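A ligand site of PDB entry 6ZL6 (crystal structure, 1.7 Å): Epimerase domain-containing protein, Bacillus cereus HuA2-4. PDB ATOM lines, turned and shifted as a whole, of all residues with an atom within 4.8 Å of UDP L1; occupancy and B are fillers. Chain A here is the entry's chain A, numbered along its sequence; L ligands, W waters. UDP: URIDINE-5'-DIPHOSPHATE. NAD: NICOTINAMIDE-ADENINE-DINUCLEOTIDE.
The guanidinium group (NE) of Arg 192 sits at hydrogen-bond distance from an oxygen (O4) of UDP L1. The guanidinium group (NE) of Arg 213 is in salt-bridge range of an oxygen (O2B) of UDP L1 (2.7 Å). O2' of UDP L1 is in hydrogen-bond range of OE1 of Glu 276 (2.4 Å). O2' of UDP L1 sits at hydrogen-bond distance from NE2 of Gln 211 (3.3 Å). A nitrogen (N3) of UDP L1 lies within hydrogen-bond range of the backbone carbonyl oxygen (O) of Thr 204. The side-chain hydroxyl (OG1) of Thr 204 sits at hydrogen-bond distance from an oxygen (O4) of UDP L1 (3.1 Å). SD of Met 188 is in hydrogen-bond range of N7N of NAD L2, at 3.7 Å. An oxygen (O2) of UDP L1 lies within hydrogen-bond range of the backbone NH (N) of Phe 206, at 3.0 Å. An oxygen (O2A) of UDP L1 is in hydrogen-bond range of the backbone NH (N) of Ala 189, at 3.3 Å. The side-chain hydroxyl (OG1) of Thr 178 lies within hydrogen-bond range of an oxygen (O2B) of UDP L1, 3.2 Å away.
The side-chain sulfur (SD) of Met 188 lies close to the side-chain amide oxygen (OE1) of Gln 184. The backbone carbonyl oxygen (O) of Phe 206 sits at hydrogen-bond distance from the side-chain amide nitrogen (NE2) of Gln 211, at 2.6 Å. The backbone carbonyl oxygen of Gln 211 sits at hydrogen-bond distance from the backbone NH of Ile 250, at 3.2 Å. OG1 of Thr 204 is in hydrogen-bond range of NH2 of Arg 192, at 2.9 Å.
Merely in contact with UDP L1: Met 188, Ile 205 and Ile 250. Hydrophobic or aromatic side chains within 4 Å of UDP L1: Met 188, Ala 189, Phe 206 and Ile 250. Of the 17 residues printed, 11 come within 4 Å of UDP L1. The nearest printed residue that does not touch UDP L1 is Phe 215 (4.3 Å).
Water W2 lies within hydrogen-bond range of O2A of UDP L1 (2.5 Å), OE1 of Gln 184 (2.9 Å) and N of Phe 190 (3.1 Å). Water W1 bridges the guanidinium group (NH2) of Arg 213 (2.8 Å) and an oxygen (O1B) of UDP L1 (3.1 Å).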
ATOM      1  N   VAL A  87     -26.868  28.479 -23.158  1.00  0.00           N
ATOM      2  CA  VAL A  87     -28.259  28.798 -22.723  1.00  0.00           C
ATOM      3  C   VAL A  87     -28.268  29.311 -21.279  1.00  0.00           C
ATOM      4  O   VAL A  87     -28.913  30.363 -21.041  1.00  0.00           O
ATOM      5  CB  VAL A  87     -29.178  27.578 -22.921  1.00  0.00           C
ATOM      6  CG1 VAL A  87     -30.589  27.876 -22.435  1.00  0.00           C
ATOM      7  CG2 VAL A  87     -29.187  27.081 -24.362  1.00  0.00           C
ATOM      8  N   THR A 178     -26.864  20.821 -32.310  1.00  0.00           N
ATOM      9  CA  THR A 178     -25.937  20.277 -31.289  1.00  0.00           C
ATOM     10  C   THR A 178     -24.778  19.467 -31.885  1.00  0.00           C
ATOM     11  O   THR A 178     -24.831  18.245 -31.958  1.00  0.00           O
ATOM     12  CB  THR A 178     -26.662  19.467 -30.224  1.00  0.00           C
ATOM     13  OG1 THR A 178     -27.849  20.177 -29.851  1.00  0.00           O
ATOM     14  CG2 THR A 178     -25.773  19.285 -29.018  1.00  0.00           C
ATOM     15  N   GLN A 184     -14.880  19.440 -28.737  1.00  0.00           N
ATOM     16  CA  GLN A 184     -16.163  19.998 -28.242  1.00  0.00           C
ATOM     17  C   GLN A 184     -15.873  20.926 -27.046  1.00  0.00           C
ATOM     18  O   GLN A 184     -15.018  20.603 -26.179  1.00  0.00           O
ATOM     19  CB  GLN A 184     -17.168  18.894 -27.902  1.00  0.00           C
ATOM     20  CG  GLN A 184     -18.592  19.447 -27.727  1.00  0.00           C
ATOM     21  CD  GLN A 184     -19.579  18.432 -27.189  1.00  0.00           C
ATOM     22  OE1 GLN A 184     -20.721  18.375 -27.669  1.00  0.00           O
ATOM     23  NE2 GLN A 184     -19.185  17.631 -26.222  1.00  0.00           N
ATOM     24  N   ASP A 187     -18.319  23.220 -21.900  1.00  0.00           N
ATOM     25  CA  ASP A 187     -19.638  23.475 -21.274  1.00  0.00           C
ATOM     26  C   ASP A 187     -20.711  22.589 -21.912  1.00  0.00           C
ATOM     27  O   ASP A 187     -21.805  22.546 -21.324  1.00  0.00           O
ATOM     28  CB  ASP A 187     -20.057  24.945 -21.376  1.00  0.00           C
ATOM     29  CG  ASP A 187     -20.207  25.402 -22.814  1.00  0.00           C
ATOM     30  OD1 ASP A 187     -19.279  25.102 -23.658  1.00  0.00           O
ATOM     31  OD2 ASP A 187     -21.197  26.100 -23.095  1.00  0.00           O
ATOM     32  N   MET A 188     -20.413  21.862 -22.985  1.00  0.00           N
ATOM     33  CA  MET A 188     -21.430  21.010 -23.664  1.00  0.00           C
ATOM     34  C   MET A 188     -21.543  19.652 -22.971  1.00  0.00           C
ATOM     35  O   MET A 188     -20.636  19.242 -22.245  1.00  0.00           O
ATOM     36  CB  MET A 188     -21.131  20.820 -25.160  1.00  0.00           C
ATOM     37  CG  MET A 188     -21.063  22.184 -25.858  1.00  0.00           C
ATOM     38  SD  MET A 188     -21.070  22.052 -27.671  1.00  0.00           S
ATOM     39  CE  MET A 188     -22.718  21.397 -27.956  1.00  0.00           C
ATOM     40  N   ALA A 189     -22.681  18.978 -23.174  1.00  0.00           N
ATOM     41  CA  ALA A 189     -23.073  17.779 -22.397  1.00  0.00           C
ATOM     42  C   ALA A 189     -22.044  16.681 -22.576  1.00  0.00           C
ATOM     43  O   ALA A 189     -21.592  16.139 -21.554  1.00  0.00           O
ATOM     44  CB  ALA A 189     -24.448  17.329 -22.830  1.00  0.00           C
ATOM     45  N   PHE A 190     -21.618  16.341 -23.784  1.00  0.00           N
ATOM     46  CA  PHE A 190     -20.789  15.137 -23.948  1.00  0.00           C
ATOM     47  C   PHE A 190     -19.411  15.365 -23.313  1.00  0.00           C
ATOM     48  O   PHE A 190     -18.889  14.471 -22.658  1.00  0.00           O
ATOM     49  CB  PHE A 190     -20.656  14.733 -25.414  1.00  0.00           C
ATOM     50  CG  PHE A 190     -21.922  14.281 -26.090  1.00  0.00           C
ATOM     51  CD1 PHE A 190     -23.144  14.270 -25.446  1.00  0.00           C
ATOM     52  CD2 PHE A 190     -21.874  13.976 -27.431  1.00  0.00           C
ATOM     53  CE1 PHE A 190     -24.290  13.904 -26.139  1.00  0.00           C
ATOM     54  CE2 PHE A 190     -23.015  13.582 -28.111  1.00  0.00           C
ATOM     55  CZ  PHE A 190     -24.209  13.543 -27.454  1.00  0.00           C
ATOM     56  N   ARG A 192     -18.708  17.332 -20.734  1.00  0.00           N
ATOM     57  CA  ARG A 192     -18.904  17.280 -19.268  1.00  0.00           C
ATOM     58  C   ARG A 192     -19.064  15.831 -18.817  1.00  0.00           C
ATOM     59  O   ARG A 192     -18.407  15.388 -17.818  1.00  0.00           O
ATOM     60  CB  ARG A 192     -20.102  18.128 -18.835  1.00  0.00           C
ATOM     61  CG  ARG A 192     -19.800  19.621 -18.939  1.00  0.00           C
ATOM     62  CD  ARG A 192     -20.999  20.513 -18.694  1.00  0.00           C
ATOM     63  NE  ARG A 192     -21.702  20.145 -17.479  1.00  0.00           N
ATOM     64  CZ  ARG A 192     -21.375  20.503 -16.235  1.00  0.00           C
ATOM     65  NH1 ARG A 192     -20.394  21.348 -16.001  1.00  0.00           N
ATOM     66  NH2 ARG A 192     -22.084  20.057 -15.236  1.00  0.00           N
ATOM     67  N   LEU A 193     -19.928  15.090 -19.473  1.00  0.00           N
ATOM     68  CA  LEU A 193     -20.299  13.733 -19.014  1.00  0.00           C
ATOM     69  C   LEU A 193     -19.100  12.797 -19.175  1.00  0.00           C
ATOM     70  O   LEU A 193     -18.880  11.928 -18.285  1.00  0.00           O
ATOM     71  CB  LEU A 193     -21.489  13.194 -19.801  1.00  0.00           C
ATOM     72  CG  LEU A 193     -22.803  13.905 -19.552  1.00  0.00           C
ATOM     73  CD1 LEU A 193     -23.811  13.516 -20.629  1.00  0.00           C
ATOM     74  CD2 LEU A 193     -23.368  13.652 -18.164  1.00  0.00           C
ATOM     75  N   THR A 204     -23.659  14.777 -14.333  1.00  0.00           N
ATOM     76  CA  THR A 204     -24.710  15.802 -14.070  1.00  0.00           C
ATOM     77  C   THR A 204     -25.740  15.742 -15.190  1.00  0.00           C
ATOM     78  O   THR A 204     -25.393  15.989 -16.368  1.00  0.00           O
ATOM     79  CB  THR A 204     -24.121  17.215 -13.911  1.00  0.00           C
ATOM     80  OG1 THR A 204     -23.357  17.477 -15.095  1.00  0.00           O
ATOM     81  CG2 THR A 204     -23.251  17.348 -12.674  1.00  0.00           C
ATOM     82  N   ILE A 205     -26.974  15.389 -14.838  1.00  0.00           N
ATOM     83  CA  ILE A 205     -28.121  15.388 -15.757  1.00  0.00           C
ATOM     84  C   ILE A 205     -29.064  16.532 -15.372  1.00  0.00           C
ATOM     85  O   ILE A 205     -29.531  16.581 -14.209  1.00  0.00           O
ATOM     86  CB  ILE A 205     -28.785  14.003 -15.707  1.00  0.00           C
ATOM     87  CG1 ILE A 205     -27.743  12.900 -15.993  1.00  0.00           C
ATOM     88  CG2 ILE A 205     -29.973  13.964 -16.662  1.00  0.00           C
ATOM     89  CD1 ILE A 205     -28.199  11.505 -15.716  1.00  0.00           C
ATOM     90  N   PHE A 206     -29.327  17.446 -16.315  1.00  0.00           N
ATOM     91  CA  PHE A 206     -30.280  18.578 -16.133  1.00  0.00           C
ATOM     92  C   PHE A 206     -31.678  18.075 -16.504  1.00  0.00           C
ATOM     93  O   PHE A 206     -31.954  17.735 -17.688  1.00  0.00           O
ATOM     94  CB  PHE A 206     -29.816  19.831 -16.885  1.00  0.00           C
ATOM     95  CG  PHE A 206     -28.391  20.253 -16.617  1.00  0.00           C
ATOM     96  CD1 PHE A 206     -27.848  20.207 -15.334  1.00  0.00           C
ATOM     97  CD2 PHE A 206     -27.567  20.679 -17.645  1.00  0.00           C
ATOM     98  CE1 PHE A 206     -26.536  20.567 -15.096  1.00  0.00           C
ATOM     99  CE2 PHE A 206     -26.259  21.052 -17.407  1.00  0.00           C
ATOM    100  CZ  PHE A 206     -25.731  20.994 -16.136  1.00  0.00           C
ATOM    101  N   GLN A 211     -34.699  14.266 -22.316  1.00  0.00           N
ATOM    102  CA  GLN A 211     -34.634  15.254 -23.403  1.00  0.00           C
ATOM    103  C   GLN A 211     -33.777  14.681 -24.534  1.00  0.00           C
ATOM    104  O   GLN A 211     -32.826  13.902 -24.249  1.00  0.00           O
ATOM    105  CB  GLN A 211     -34.065  16.587 -22.917  1.00  0.00           C
ATOM    106  CG  GLN A 211     -32.658  16.459 -22.372  1.00  0.00           C
ATOM    107  CD  GLN A 211     -32.647  16.441 -20.867  1.00  0.00           C
ATOM    108  OE1 GLN A 211     -33.345  15.661 -20.241  1.00  0.00           O
ATOM    109  NE2 GLN A 211     -31.831  17.277 -20.268  1.00  0.00           N
ATOM    110  N   ARG A 213     -31.769  15.331 -28.512  1.00  0.00           N
ATOM    111  CA  ARG A 213     -31.161  16.258 -29.474  1.00  0.00           C
ATOM    112  C   ARG A 213     -30.857  15.555 -30.772  1.00  0.00           C
ATOM    113  O   ARG A 213     -30.499  14.385 -30.770  1.00  0.00           O
ATOM    114  CB  ARG A 213     -29.871  16.882 -28.924  1.00  0.00           C
ATOM    115  CG  ARG A 213     -30.058  17.737 -27.675  1.00  0.00           C
ATOM    116  CD  ARG A 213     -30.693  19.065 -28.021  1.00  0.00           C
ATOM    117  NE  ARG A 213     -30.846  19.990 -26.889  1.00  0.00           N
ATOM    118  CZ  ARG A 213     -31.895  20.070 -26.085  1.00  0.00           C
ATOM    119  NH1 ARG A 213     -32.937  19.271 -26.280  1.00  0.00           N
ATOM    120  NH2 ARG A 213     -31.935  20.995 -25.136  1.00  0.00           N
ATOM    121  N   PHE A 215     -28.086  15.282 -32.570  1.00  0.00           N
ATOM    122  CA  PHE A 215     -26.622  15.455 -32.366  1.00  0.00           C
ATOM    123  C   PHE A 215     -25.903  15.275 -33.699  1.00  0.00           C
ATOM    124  O   PHE A 215     -26.207  14.352 -34.464  1.00  0.00           O
ATOM    125  CB  PHE A 215     -26.094  14.461 -31.334  1.00  0.00           C
ATOM    126  CG  PHE A 215     -26.609  14.629 -29.938  1.00  0.00           C
ATOM    127  CD1 PHE A 215     -26.175  15.694 -29.145  1.00  0.00           C
ATOM    128  CD2 PHE A 215     -27.465  13.704 -29.354  1.00  0.00           C
ATOM    129  CE1 PHE A 215     -26.609  15.837 -27.838  1.00  0.00           C
ATOM    130  CE2 PHE A 215     -27.890  13.850 -28.045  1.00  0.00           C
ATOM    131  CZ  PHE A 215     -27.479  14.922 -27.288  1.00  0.00           C
ATOM    132  N   ILE A 250     -30.339  12.045 -23.388  1.00  0.00           N
ATOM    133  CA  ILE A 250     -29.141  12.093 -22.510  1.00  0.00           C
ATOM    134  C   ILE A 250     -29.008  10.715 -21.838  1.00  0.00           C
ATOM    135  O   ILE A 250     -27.890  10.209 -21.754  1.00  0.00           O
ATOM    136  CB  ILE A 250     -29.210  13.286 -21.552  1.00  0.00           C
ATOM    137  CG1 ILE A 250     -29.075  14.583 -22.355  1.00  0.00           C
ATOM    138  CG2 ILE A 250     -28.165  13.186 -20.442  1.00  0.00           C
ATOM    139  CD1 ILE A 250     -27.728  14.734 -22.989  1.00  0.00           C
ATOM    140  N   GLU A 276     -34.169  25.831 -22.134  1.00  0.00           N
ATOM    141  CA  GLU A 276     -33.749  24.662 -22.969  1.00  0.00           C
ATOM    142  C   GLU A 276     -34.991  23.950 -23.470  1.00  0.00           C
ATOM    143  O   GLU A 276     -35.853  23.630 -22.650  1.00  0.00           O
ATOM    144  CB  GLU A 276     -32.955  23.623 -22.177  1.00  0.00           C
ATOM    145  CG  GLU A 276     -31.575  24.097 -21.821  1.00  0.00           C
ATOM    146  CD  GLU A 276     -30.674  22.973 -21.316  1.00  0.00           C
ATOM    147  OE1 GLU A 276     -31.192  22.022 -20.692  1.00  0.00           O
ATOM    148  OE2 GLU A 276     -29.466  23.086 -21.498  1.00  0.00           O
HETATM  149  N1  UDP L   1     -27.027  18.546 -20.281  1.00  0.00           N
HETATM  150  C2  UDP L   1     -26.976  17.636 -19.191  1.00  0.00           C
HETATM  151  N3  UDP L   1     -25.869  17.570 -18.460  1.00  0.00           N
HETATM  152  C4  UDP L   1     -24.848  18.397 -18.688  1.00  0.00           C
HETATM  153  C5  UDP L   1     -24.907  19.319 -19.764  1.00  0.00           C
HETATM  154  C6  UDP L   1     -26.012  19.363 -20.549  1.00  0.00           C
HETATM  155  O2  UDP L   1     -27.945  16.887 -18.970  1.00  0.00           O
HETATM  156  O4  UDP L   1     -23.850  18.398 -17.966  1.00  0.00           O
HETATM  157  C1' UDP L   1     -28.207  18.504 -21.153  1.00  0.00           C
HETATM  158  C2' UDP L   1     -28.825  19.845 -21.500  1.00  0.00           C
HETATM  159  O2' UDP L   1     -29.984  19.932 -20.668  1.00  0.00           O
HETATM  160  C3' UDP L   1     -29.295  19.609 -22.914  1.00  0.00           C
HETATM  161  C4' UDP L   1     -28.458  18.465 -23.454  1.00  0.00           C
HETATM  162  O4' UDP L   1     -27.706  17.914 -22.356  1.00  0.00           O
HETATM  163  O3' UDP L   1     -30.668  19.102 -22.866  1.00  0.00           O
HETATM  164  C5' UDP L   1     -27.553  18.828 -24.568  1.00  0.00           C
HETATM  165  O5' UDP L   1     -26.801  19.940 -24.139  1.00  0.00           O
HETATM  166  PA  UDP L   1     -25.500  20.298 -25.031  1.00  0.00           P
HETATM  167  O1A UDP L   1     -24.851  21.287 -24.171  1.00  0.00           O
HETATM  168  O2A UDP L   1     -24.847  19.090 -25.687  1.00  0.00           O
HETATM  169  O3A UDP L   1     -26.127  21.055 -26.296  1.00  0.00           O
HETATM  170  PB  UDP L   1     -27.364  22.103 -26.526  1.00  0.00           P
HETATM  171  O1B UDP L   1     -27.472  22.969 -25.329  1.00  0.00           O
HETATM  172  O2B UDP L   1     -28.529  21.336 -26.929  1.00  0.00           O
HETATM  173  O3B UDP L   1     -26.749  22.912 -27.659  1.00  0.00           O
HETATM  174  PA  NAD L   2     -16.730  28.376 -29.547  1.00  0.00           P
HETATM  175  O1A NAD L   2     -15.819  27.217 -29.389  1.00  0.00           O
HETATM  176  O2A NAD L   2     -16.994  29.197 -28.331  1.00  0.00           O
HETATM  177  O5B NAD L   2     -16.207  29.236 -30.797  1.00  0.00           O
HETATM  178  C5B NAD L   2     -16.599  30.587 -31.102  1.00  0.00           C
HETATM  179  C4B NAD L   2     -15.400  31.506 -31.008  1.00  0.00           C
HETATM  180  O4B NAD L   2     -15.860  32.857 -31.236  1.00  0.00           O
HETATM  181  C3B NAD L   2     -14.649  31.524 -29.653  1.00  0.00           C
HETATM  182  O3B NAD L   2     -13.401  30.822 -29.772  1.00  0.00           O
HETATM  183  C2B NAD L   2     -14.550  33.025 -29.327  1.00  0.00           C
HETATM  184  O2B NAD L   2     -13.290  33.399 -28.793  1.00  0.00           O
HETATM  185  C1B NAD L   2     -14.866  33.679 -30.662  1.00  0.00           C
HETATM  186  N9A NAD L   2     -15.385  35.026 -30.553  1.00  0.00           N
HETATM  187  C8A NAD L   2     -16.509  35.378 -29.848  1.00  0.00           C
HETATM  188  N7A NAD L   2     -16.741  36.659 -29.842  1.00  0.00           N
HETATM  189  C5A NAD L   2     -15.684  37.218 -30.564  1.00  0.00           C
HETATM  190  C6A NAD L   2     -15.338  38.561 -30.892  1.00  0.00           C
HETATM  191  N6A NAD L   2     -16.028  39.612 -30.474  1.00  0.00           N
HETATM  192  N1A NAD L   2     -14.187  38.756 -31.583  1.00  0.00           N
HETATM  193  C2A NAD L   2     -13.480  37.673 -31.947  1.00  0.00           C
HETATM  194  N3A NAD L   2     -13.691  36.377 -31.681  1.00  0.00           N
HETATM  195  C4A NAD L   2     -14.833  36.214 -30.984  1.00  0.00           C
HETATM  196  O3  NAD L   2     -18.197  27.872 -30.048  1.00  0.00           O
HETATM  197  PN  NAD L   2     -18.532  26.772 -31.192  1.00  0.00           P
HETATM  198  O1N NAD L   2     -17.370  26.477 -32.087  1.00  0.00           O
HETATM  199  O2N NAD L   2     -19.209  25.640 -30.460  1.00  0.00           O
HETATM  200  O5D NAD L   2     -19.649  27.491 -32.045  1.00  0.00           O
HETATM  201  C5D NAD L   2     -19.339  28.076 -33.298  1.00  0.00           C
HETATM  202  C4D NAD L   2     -20.594  28.689 -33.875  1.00  0.00           C
HETATM  203  O4D NAD L   2     -21.579  27.656 -34.104  1.00  0.00           O
HETATM  204  C3D NAD L   2     -21.269  29.741 -32.974  1.00  0.00           C
HETATM  205  O3D NAD L   2     -21.722  30.770 -33.826  1.00  0.00           O
HETATM  206  C2D NAD L   2     -22.423  28.969 -32.313  1.00  0.00           C
HETATM  207  O2D NAD L   2     -23.451  29.860 -31.975  1.00  0.00           O
HETATM  208  C1D NAD L   2     -22.773  28.036 -33.483  1.00  0.00           C
HETATM  209  N1N NAD L   2     -23.411  26.796 -33.074  1.00  0.00           N
HETATM  210  C2N NAD L   2     -22.710  25.806 -32.428  1.00  0.00           C
HETATM  211  C3N NAD L   2     -23.338  24.660 -31.978  1.00  0.00           C
HETATM  212  C7N NAD L   2     -22.602  23.608 -31.196  1.00  0.00           C
HETATM  213  O7N NAD L   2     -23.252  22.625 -30.892  1.00  0.00           O
HETATM  214  N7N NAD L   2     -21.311  23.813 -30.860  1.00  0.00           N
HETATM  215  C4N NAD L   2     -24.708  24.481 -32.268  1.00  0.00           C
HETATM  216  C5N NAD L   2     -25.388  25.470 -32.944  1.00  0.00           C
HETATM  217  C6N NAD L   2     -24.720  26.578 -33.409  1.00  0.00           C
HETATM  218  O   HOH W   1     -30.478  23.386 -24.844  1.00  0.00           O
HETATM  219  O   HOH W   2     -23.052  17.406 -26.302  1.00  0.00           O
HETATM  220  O   HOH W   3     -25.900  25.260 -24.622  1.00  0.00           O
